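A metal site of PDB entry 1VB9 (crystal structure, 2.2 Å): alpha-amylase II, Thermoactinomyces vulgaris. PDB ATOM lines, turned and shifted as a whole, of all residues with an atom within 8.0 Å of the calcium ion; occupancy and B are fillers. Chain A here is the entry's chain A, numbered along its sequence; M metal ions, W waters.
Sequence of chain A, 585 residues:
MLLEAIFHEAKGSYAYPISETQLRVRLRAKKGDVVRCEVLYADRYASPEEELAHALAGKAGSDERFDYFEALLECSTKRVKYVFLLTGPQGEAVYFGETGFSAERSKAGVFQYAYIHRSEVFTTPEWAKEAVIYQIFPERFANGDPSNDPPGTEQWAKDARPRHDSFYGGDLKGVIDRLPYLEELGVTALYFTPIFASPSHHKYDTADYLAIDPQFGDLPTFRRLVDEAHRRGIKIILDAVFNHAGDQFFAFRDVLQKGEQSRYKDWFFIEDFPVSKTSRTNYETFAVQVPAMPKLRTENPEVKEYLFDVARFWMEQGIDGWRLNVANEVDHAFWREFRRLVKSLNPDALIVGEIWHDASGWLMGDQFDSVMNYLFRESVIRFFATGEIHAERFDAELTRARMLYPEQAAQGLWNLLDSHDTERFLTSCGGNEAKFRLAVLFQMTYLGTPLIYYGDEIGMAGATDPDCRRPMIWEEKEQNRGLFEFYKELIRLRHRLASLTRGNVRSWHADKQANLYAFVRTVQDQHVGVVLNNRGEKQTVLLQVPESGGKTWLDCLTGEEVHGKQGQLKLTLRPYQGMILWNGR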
ATOM      1  N   PRO A 138       8.789  14.729   3.662  1.00  0.00           N
ATOM      2  CA  PRO A 138       8.738  14.182   2.295  1.00  0.00           C
ATOM      3  C   PRO A 138       8.259  15.063   1.144  1.00  0.00           C
ATOM      4  O   PRO A 138       8.896  15.095   0.092  1.00  0.00           O
ATOM      5  CB  PRO A 138       7.877  12.924   2.455  1.00  0.00           C
ATOM      6  CG  PRO A 138       8.143  12.518   3.859  1.00  0.00           C
ATOM      7  CD  PRO A 138       8.059  13.830   4.578  1.00  0.00           C
ATOM      8  N   GLU A 139       7.135  15.745   1.317  1.00  0.00           N
ATOM      9  CA  GLU A 139       6.603  16.588   0.243  1.00  0.00           C
ATOM     10  C   GLU A 139       7.578  17.695  -0.130  1.00  0.00           C
ATOM     11  O   GLU A 139       7.494  18.282  -1.212  1.00  0.00           O
ATOM     12  CB  GLU A 139       5.256  17.186   0.668  1.00  0.00           C
ATOM     13  CG  GLU A 139       4.153  17.103  -0.403  1.00  0.00           C
ATOM     14  CD  GLU A 139       4.416  17.997  -1.616  1.00  0.00           C
ATOM     15  OE1 GLU A 139       4.231  17.517  -2.748  1.00  0.00           O
ATOM     16  OE2 GLU A 139       4.799  19.165  -1.426  1.00  0.00           O
ATOM     17  N   ALA A 142      12.987  16.124  -1.530  1.00  0.00           N
ATOM     18  CA  ALA A 142      13.532  15.923  -2.868  1.00  0.00           C
ATOM     19  C   ALA A 142      12.486  15.298  -3.790  1.00  0.00           C
ATOM     20  O   ALA A 142      11.830  14.325  -3.413  1.00  0.00           O
ATOM     21  CB  ALA A 142      14.785  15.045  -2.796  1.00  0.00           C
ATOM     22  N   ASN A 143      12.335  15.864  -4.978  1.00  0.00           N
ATOM     23  CA  ASN A 143      11.383  15.351  -5.957  1.00  0.00           C
ATOM     24  C   ASN A 143      12.186  14.492  -6.925  1.00  0.00           C
ATOM     25  O   ASN A 143      12.717  14.994  -7.918  1.00  0.00           O
ATOM     26  CB  ASN A 143      10.706  16.502  -6.707  1.00  0.00           C
ATOM     27  CG  ASN A 143       9.664  16.009  -7.697  1.00  0.00           C
ATOM     28  OD1 ASN A 143       9.496  14.812  -7.900  1.00  0.00           O
ATOM     29  ND2 ASN A 143       8.944  16.946  -8.314  1.00  0.00           N
ATOM     30  N   GLY A 144      12.273  13.199  -6.622  1.00  0.00           N
ATOM     31  CA  GLY A 144      13.030  12.290  -7.479  1.00  0.00           C
ATOM     32  C   GLY A 144      12.224  11.732  -8.634  1.00  0.00           C
ATOM     33  O   GLY A 144      12.792  11.239  -9.612  1.00  0.00           O
ATOM     34  N   ASP A 145      10.901  11.820  -8.539  1.00  0.00           N
ATOM     35  CA  ASP A 145      10.011  11.309  -9.569  1.00  0.00           C
ATOM     36  C   ASP A 145       8.920  12.331  -9.881  1.00  0.00           C
ATOM     37  O   ASP A 145       7.884  12.396  -9.204  1.00  0.00           O
ATOM     38  CB  ASP A 145       9.379   9.995  -9.112  1.00  0.00           C
ATOM     39  CG  ASP A 145       8.436   9.397 -10.133  1.00  0.00           C
ATOM     40  OD1 ASP A 145       8.305   9.951 -11.251  1.00  0.00           O
ATOM     41  OD2 ASP A 145       7.824   8.351  -9.819  1.00  0.00           O
ATOM     42  N   PRO A 146       9.133  13.156 -10.914  1.00  0.00           N
ATOM     43  CA  PRO A 146       8.169  14.187 -11.306  1.00  0.00           C
ATOM     44  C   PRO A 146       6.832  13.647 -11.833  1.00  0.00           C
ATOM     45  O   PRO A 146       5.863  14.402 -11.935  1.00  0.00           O
ATOM     46  CB  PRO A 146       8.926  14.979 -12.373  1.00  0.00           C
ATOM     47  CG  PRO A 146       9.747  13.931 -13.022  1.00  0.00           C
ATOM     48  CD  PRO A 146      10.283  13.140 -11.845  1.00  0.00           C
ATOM     49  N   SER A 147       6.793  12.355 -12.152  1.00  0.00           N
ATOM     50  CA  SER A 147       5.570  11.748 -12.679  1.00  0.00           C
ATOM     51  C   SER A 147       4.497  11.423 -11.649  1.00  0.00           C
ATOM     52  O   SER A 147       3.392  11.017 -12.007  1.00  0.00           O
ATOM     53  CB  SER A 147       5.894  10.485 -13.470  1.00  0.00           C
ATOM     54  OG  SER A 147       6.158   9.387 -12.602  1.00  0.00           O
ATOM     55  N   ASN A 148       4.793  11.583 -10.351  1.00  0.00           N
ATOM     56  CA  ASN A 148       3.802  11.302  -9.318  1.00  0.00           C
ATOM     57  C   ASN A 148       3.437  12.575  -8.561  1.00  0.00           C
ATOM     58  O   ASN A 148       2.788  12.511  -7.518  1.00  0.00           O
ATOM     59  CB  ASN A 148       4.327  10.254  -8.316  1.00  0.00           C
ATOM     60  CG  ASN A 148       5.555  10.727  -7.537  1.00  0.00           C
ATOM     61  OD1 ASN A 148       5.813  11.919  -7.429  1.00  0.00           O
ATOM     62  ND2 ASN A 148       6.300   9.776  -6.971  1.00  0.00           N
ATOM     63  N   ASP A 149       3.849  13.714  -9.091  1.00  0.00           N
ATOM     64  CA  ASP A 149       3.565  14.987  -8.442  1.00  0.00           C
ATOM     65  C   ASP A 149       2.076  15.261  -8.357  1.00  0.00           C
ATOM     66  O   ASP A 149       1.327  14.962  -9.274  1.00  0.00           O
ATOM     67  CB  ASP A 149       4.238  16.139  -9.196  1.00  0.00           C
ATOM     68  CG  ASP A 149       5.742  16.105  -9.092  1.00  0.00           C
ATOM     69  OD1 ASP A 149       6.393  17.030  -9.629  1.00  0.00           O
ATOM     70  OD2 ASP A 149       6.288  15.160  -8.487  1.00  0.00           O
ATOM     71  N   PRO A 150       1.625  15.845  -7.240  1.00  0.00           N
ATOM     72  CA  PRO A 150       0.202  16.144  -7.119  1.00  0.00           C
ATOM     73  C   PRO A 150      -0.146  17.238  -8.128  1.00  0.00           C
ATOM     74  O   PRO A 150       0.739  17.905  -8.661  1.00  0.00           O
ATOM     75  CB  PRO A 150       0.062  16.661  -5.687  1.00  0.00           C
ATOM     76  CG  PRO A 150       1.222  16.017  -4.971  1.00  0.00           C
ATOM     77  CD  PRO A 150       2.334  16.136  -5.982  1.00  0.00           C
ATOM     78  N   THR A 153       1.350  21.319  -8.495  1.00  0.00           N
ATOM     79  CA  THR A 153       2.689  21.383  -7.905  1.00  0.00           C
ATOM     80  C   THR A 153       3.382  22.657  -8.338  1.00  0.00           C
ATOM     81  O   THR A 153       3.425  22.974  -9.528  1.00  0.00           O
ATOM     82  CB  THR A 153       3.558  20.179  -8.326  1.00  0.00           C
ATOM     83  OG1 THR A 153       3.040  18.979  -7.735  1.00  0.00           O
ATOM     84  CG2 THR A 153       4.994  20.376  -7.891  1.00  0.00           C
ATOM     85  N   TRP A 156      10.086  24.238  -7.754  1.00  0.00           N
ATOM     86  CA  TRP A 156      11.098  24.063  -6.722  1.00  0.00           C
ATOM     87  C   TRP A 156      12.157  25.155  -6.793  1.00  0.00           C
ATOM     88  O   TRP A 156      13.067  25.089  -7.624  1.00  0.00           O
ATOM     89  CB  TRP A 156      11.740  22.688  -6.911  1.00  0.00           C
ATOM     90  CG  TRP A 156      12.347  22.102  -5.683  1.00  0.00           C
ATOM     91  CD1 TRP A 156      13.509  22.483  -5.073  1.00  0.00           C
ATOM     92  CD2 TRP A 156      11.822  21.028  -4.912  1.00  0.00           C
ATOM     93  NE1 TRP A 156      13.737  21.709  -3.959  1.00  0.00           N
ATOM     94  CE2 TRP A 156      12.720  20.803  -3.839  1.00  0.00           C
ATOM     95  CE3 TRP A 156      10.679  20.217  -5.024  1.00  0.00           C
ATOM     96  CZ2 TRP A 156      12.500  19.803  -2.877  1.00  0.00           C
ATOM     97  CZ3 TRP A 156      10.474  19.226  -4.060  1.00  0.00           C
ATOM     98  CH2 TRP A 156      11.382  19.029  -3.000  1.00  0.00           C
ATOM     99  N   TYR A 168       4.861  20.576  -3.809  1.00  0.00           N
ATOM    100  CA  TYR A 168       6.107  20.813  -4.538  1.00  0.00           C
ATOM    101  C   TYR A 168       6.644  19.557  -5.197  1.00  0.00           C
ATOM    102  O   TYR A 168       7.593  19.616  -5.984  1.00  0.00           O
ATOM    103  CB  TYR A 168       7.155  21.413  -3.596  1.00  0.00           C
ATOM    104  CG  TYR A 168       6.857  22.855  -3.224  1.00  0.00           C
ATOM    105  CD1 TYR A 168       7.244  23.910  -4.051  1.00  0.00           C
ATOM    106  CD2 TYR A 168       6.140  23.159  -2.067  1.00  0.00           C
ATOM    107  CE1 TYR A 168       6.918  25.231  -3.745  1.00  0.00           C
ATOM    108  CE2 TYR A 168       5.812  24.471  -1.740  1.00  0.00           C
ATOM    109  CZ  TYR A 168       6.203  25.511  -2.582  1.00  0.00           C
ATOM    110  OH  TYR A 168       5.858  26.808  -2.277  1.00  0.00           O
ATOM    111  N   GLY A 169       6.058  18.408  -4.863  1.00  0.00           N
ATOM    112  CA  GLY A 169       6.485  17.169  -5.484  1.00  0.00           C
ATOM    113  C   GLY A 169       7.506  16.278  -4.799  1.00  0.00           C
ATOM    114  O   GLY A 169       7.936  15.293  -5.386  1.00  0.00           O
ATOM    115  N   GLY A 170       7.897  16.611  -3.568  1.00  0.00           N
ATOM    116  CA  GLY A 170       8.865  15.777  -2.870  1.00  0.00           C
ATOM    117  C   GLY A 170       8.354  14.349  -2.764  1.00  0.00           C
ATOM    118  O   GLY A 170       7.153  14.135  -2.616  1.00  0.00           O
ATOM    119  N   ASP A 171       9.250  13.370  -2.856  1.00  0.00           N
ATOM    120  CA  ASP A 171       8.843  11.966  -2.793  1.00  0.00           C
ATOM    121  C   ASP A 171       9.924  11.051  -2.217  1.00  0.00           C
ATOM    122  O   ASP A 171      11.026  11.507  -1.898  1.00  0.00           O
ATOM    123  CB  ASP A 171       8.419  11.482  -4.185  1.00  0.00           C
ATOM    124  CG  ASP A 171       9.455  11.801  -5.250  1.00  0.00           C
ATOM    125  OD1 ASP A 171      10.655  11.518  -5.011  1.00  0.00           O
ATOM    126  OD2 ASP A 171       9.072  12.335  -6.316  1.00  0.00           O
ATOM    127  N   LEU A 172       9.618   9.762  -2.084  1.00  0.00           N
ATOM    128  CA  LEU A 172      10.564   8.802  -1.515  1.00  0.00           C
ATOM    129  C   LEU A 172      11.737   8.510  -2.432  1.00  0.00           C
ATOM    130  O   LEU A 172      12.845   8.239  -1.970  1.00  0.00           O
ATOM    131  CB  LEU A 172       9.857   7.500  -1.148  1.00  0.00           C
ATOM    132  CG  LEU A 172       8.750   7.642  -0.095  1.00  0.00           C
ATOM    133  CD1 LEU A 172       8.156   6.279   0.201  1.00  0.00           C
ATOM    134  CD2 LEU A 172       9.311   8.272   1.170  1.00  0.00           C
ATOM    135  N   LYS A 173      11.499   8.557  -3.744  1.00  0.00           N
ATOM    136  CA  LYS A 173      12.571   8.315  -4.704  1.00  0.00           C
ATOM    137  C   LYS A 173      13.593   9.419  -4.518  1.00  0.00           C
ATOM    138  O   LYS A 173      14.799   9.197  -4.650  1.00  0.00           O
ATOM    139  CB  LYS A 173      12.040   8.339  -6.133  1.00  0.00           C
ATOM    140  CG  LYS A 173      13.126   8.174  -7.187  1.00  0.00           C
ATOM    141  CD  LYS A 173      13.918   6.889  -6.996  1.00  0.00           C
ATOM    142  CE  LYS A 173      14.949   6.696  -8.101  1.00  0.00           C
ATOM    143  NZ  LYS A 173      14.284   6.667  -9.438  1.00  0.00           N
ATOM    144  N   GLY A 174      13.107  10.627  -4.211  1.00  0.00           N
ATOM    145  CA  GLY A 174      13.989  11.752  -3.992  1.00  0.00           C
ATOM    146  C   GLY A 174      14.863  11.503  -2.772  1.00  0.00           C
ATOM    147  O   GLY A 174      16.050  11.857  -2.774  1.00  0.00           O
ATOM    148  N   PRO A 214       0.507   7.562  -2.976  1.00  0.00           N
ATOM    149  CA  PRO A 214       0.836   7.511  -4.411  1.00  0.00           C
ATOM    150  C   PRO A 214       1.806   8.590  -4.893  1.00  0.00           C
ATOM    151  O   PRO A 214       2.620   8.337  -5.779  1.00  0.00           O
ATOM    152  CB  PRO A 214      -0.529   7.615  -5.087  1.00  0.00           C
ATOM    153  CG  PRO A 214      -1.408   6.878  -4.113  1.00  0.00           C
ATOM    154  CD  PRO A 214      -0.945   7.442  -2.787  1.00  0.00           C
ATOM    155  N   GLN A 215       1.714   9.787  -4.331  1.00  0.00           N
ATOM    156  CA  GLN A 215       2.587  10.882  -4.724  1.00  0.00           C
ATOM    157  C   GLN A 215       3.986  10.761  -4.100  1.00  0.00           C
ATOM    158  O   GLN A 215       4.897  11.505  -4.464  1.00  0.00           O
ATOM    159  CB  GLN A 215       1.973  12.226  -4.347  1.00  0.00           C
ATOM    160  CG  GLN A 215       2.008  12.550  -2.862  1.00  0.00           C
ATOM    161  CD  GLN A 215       1.280  13.849  -2.528  1.00  0.00           C
ATOM    162  OE1 GLN A 215       0.078  13.989  -2.757  1.00  0.00           O
ATOM    163  NE2 GLN A 215       2.020  14.817  -1.985  1.00  0.00           N
ATOM    164  N   PHE A 216       4.130   9.819  -3.168  1.00  0.00           N
ATOM    165  CA  PHE A 216       5.411   9.581  -2.501  1.00  0.00           C
ATOM    166  C   PHE A 216       6.085   8.334  -3.071  1.00  0.00           C
ATOM    167  O   PHE A 216       7.318   8.221  -3.060  1.00  0.00           O
ATOM    168  CB  PHE A 216       5.235   9.406  -0.979  1.00  0.00           C
ATOM    169  CG  PHE A 216       4.994  10.693  -0.223  1.00  0.00           C
ATOM    170  CD1 PHE A 216       5.180  11.926  -0.841  1.00  0.00           C
ATOM    171  CD2 PHE A 216       4.615  10.656   1.115  1.00  0.00           C
ATOM    172  CE1 PHE A 216       4.996  13.117  -0.122  1.00  0.00           C
ATOM    173  CE2 PHE A 216       4.431  11.847   1.834  1.00  0.00           C
ATOM    174  CZ  PHE A 216       4.627  13.076   1.215  1.00  0.00           C
ATOM    175  N   GLY A 217       5.280   7.387  -3.540  1.00  0.00           N
ATOM    176  CA  GLY A 217       5.825   6.166  -4.098  1.00  0.00           C
ATOM    177  C   GLY A 217       4.866   5.013  -3.920  1.00  0.00           C
ATOM    178  O   GLY A 217       3.643   5.186  -3.969  1.00  0.00           O
HETATM  179 CA    CA M   1       7.364  13.696  -7.201  1.00  0.00          CA
HETATM  180  O   HOH W   1       5.508  13.757  -5.721  1.00  0.00           O
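O of Pro 138 is in hydrogen-bond range of N of Asp 171, at 3.4 Å.
OG of Ser 147 lies within hydrogen-bond range of OD1 of Asp 145 (2.6 Å).
The backbone NH of Gly 144 lies within hydrogen-bond range of the side-chain carboxylate of Asp 171, 2.8 Å away.
OD1 of Asp 171 sits close to N of Lys 173, at 3.3 Å.
N of Gly 174 is in hydrogen-bond range of OD1 of Asp 171.
The backbone NH (N) of Asp 171 is in hydrogen-bond range of the backbone carbonyl oxygen (O) of Ala 142, at 2.8 Å.
ND2 of Asn 148 lies close to O of Gln 215 (3.4 Å).
N of Gly 169 is in hydrogen-bond range of OE1 of Glu 139.
Of the 24 residues printed, 6 come within 4 Å of the calcium ion.
Along chain A the residues within 4 Å of the calcium ion span positions 143 to 171.
The nearest printed residue that does not touch the calcium ion is Pro 146 (4.1 Å).
Water W1 lies within hydrogen-bond range of O of Gln 215 (2.7 Å) and O of Asn 148 (3.5 Å).
The side-chain carboxylate (OD2) of Asp 149 is bound to the calcium ion (2.2 Å).
The side-chain carboxylate (OD2) of Asp 171 binds the calcium ion, 2.4 Å away.
The calcium ion is bound by OD1 of Asn 148 (2.4 Å).
The calcium ion is bound by water W1.
O of Asp 145 is bound to the calcium ion, at 2.4 Å.
O of Gly 169 is bound to the calcium ion (2.5 Å).
The side-chain amide oxygen (OD1) of Asn 143 binds the calcium ion (2.5 Å).
The calcium ion has seven donor atoms within binding distance.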
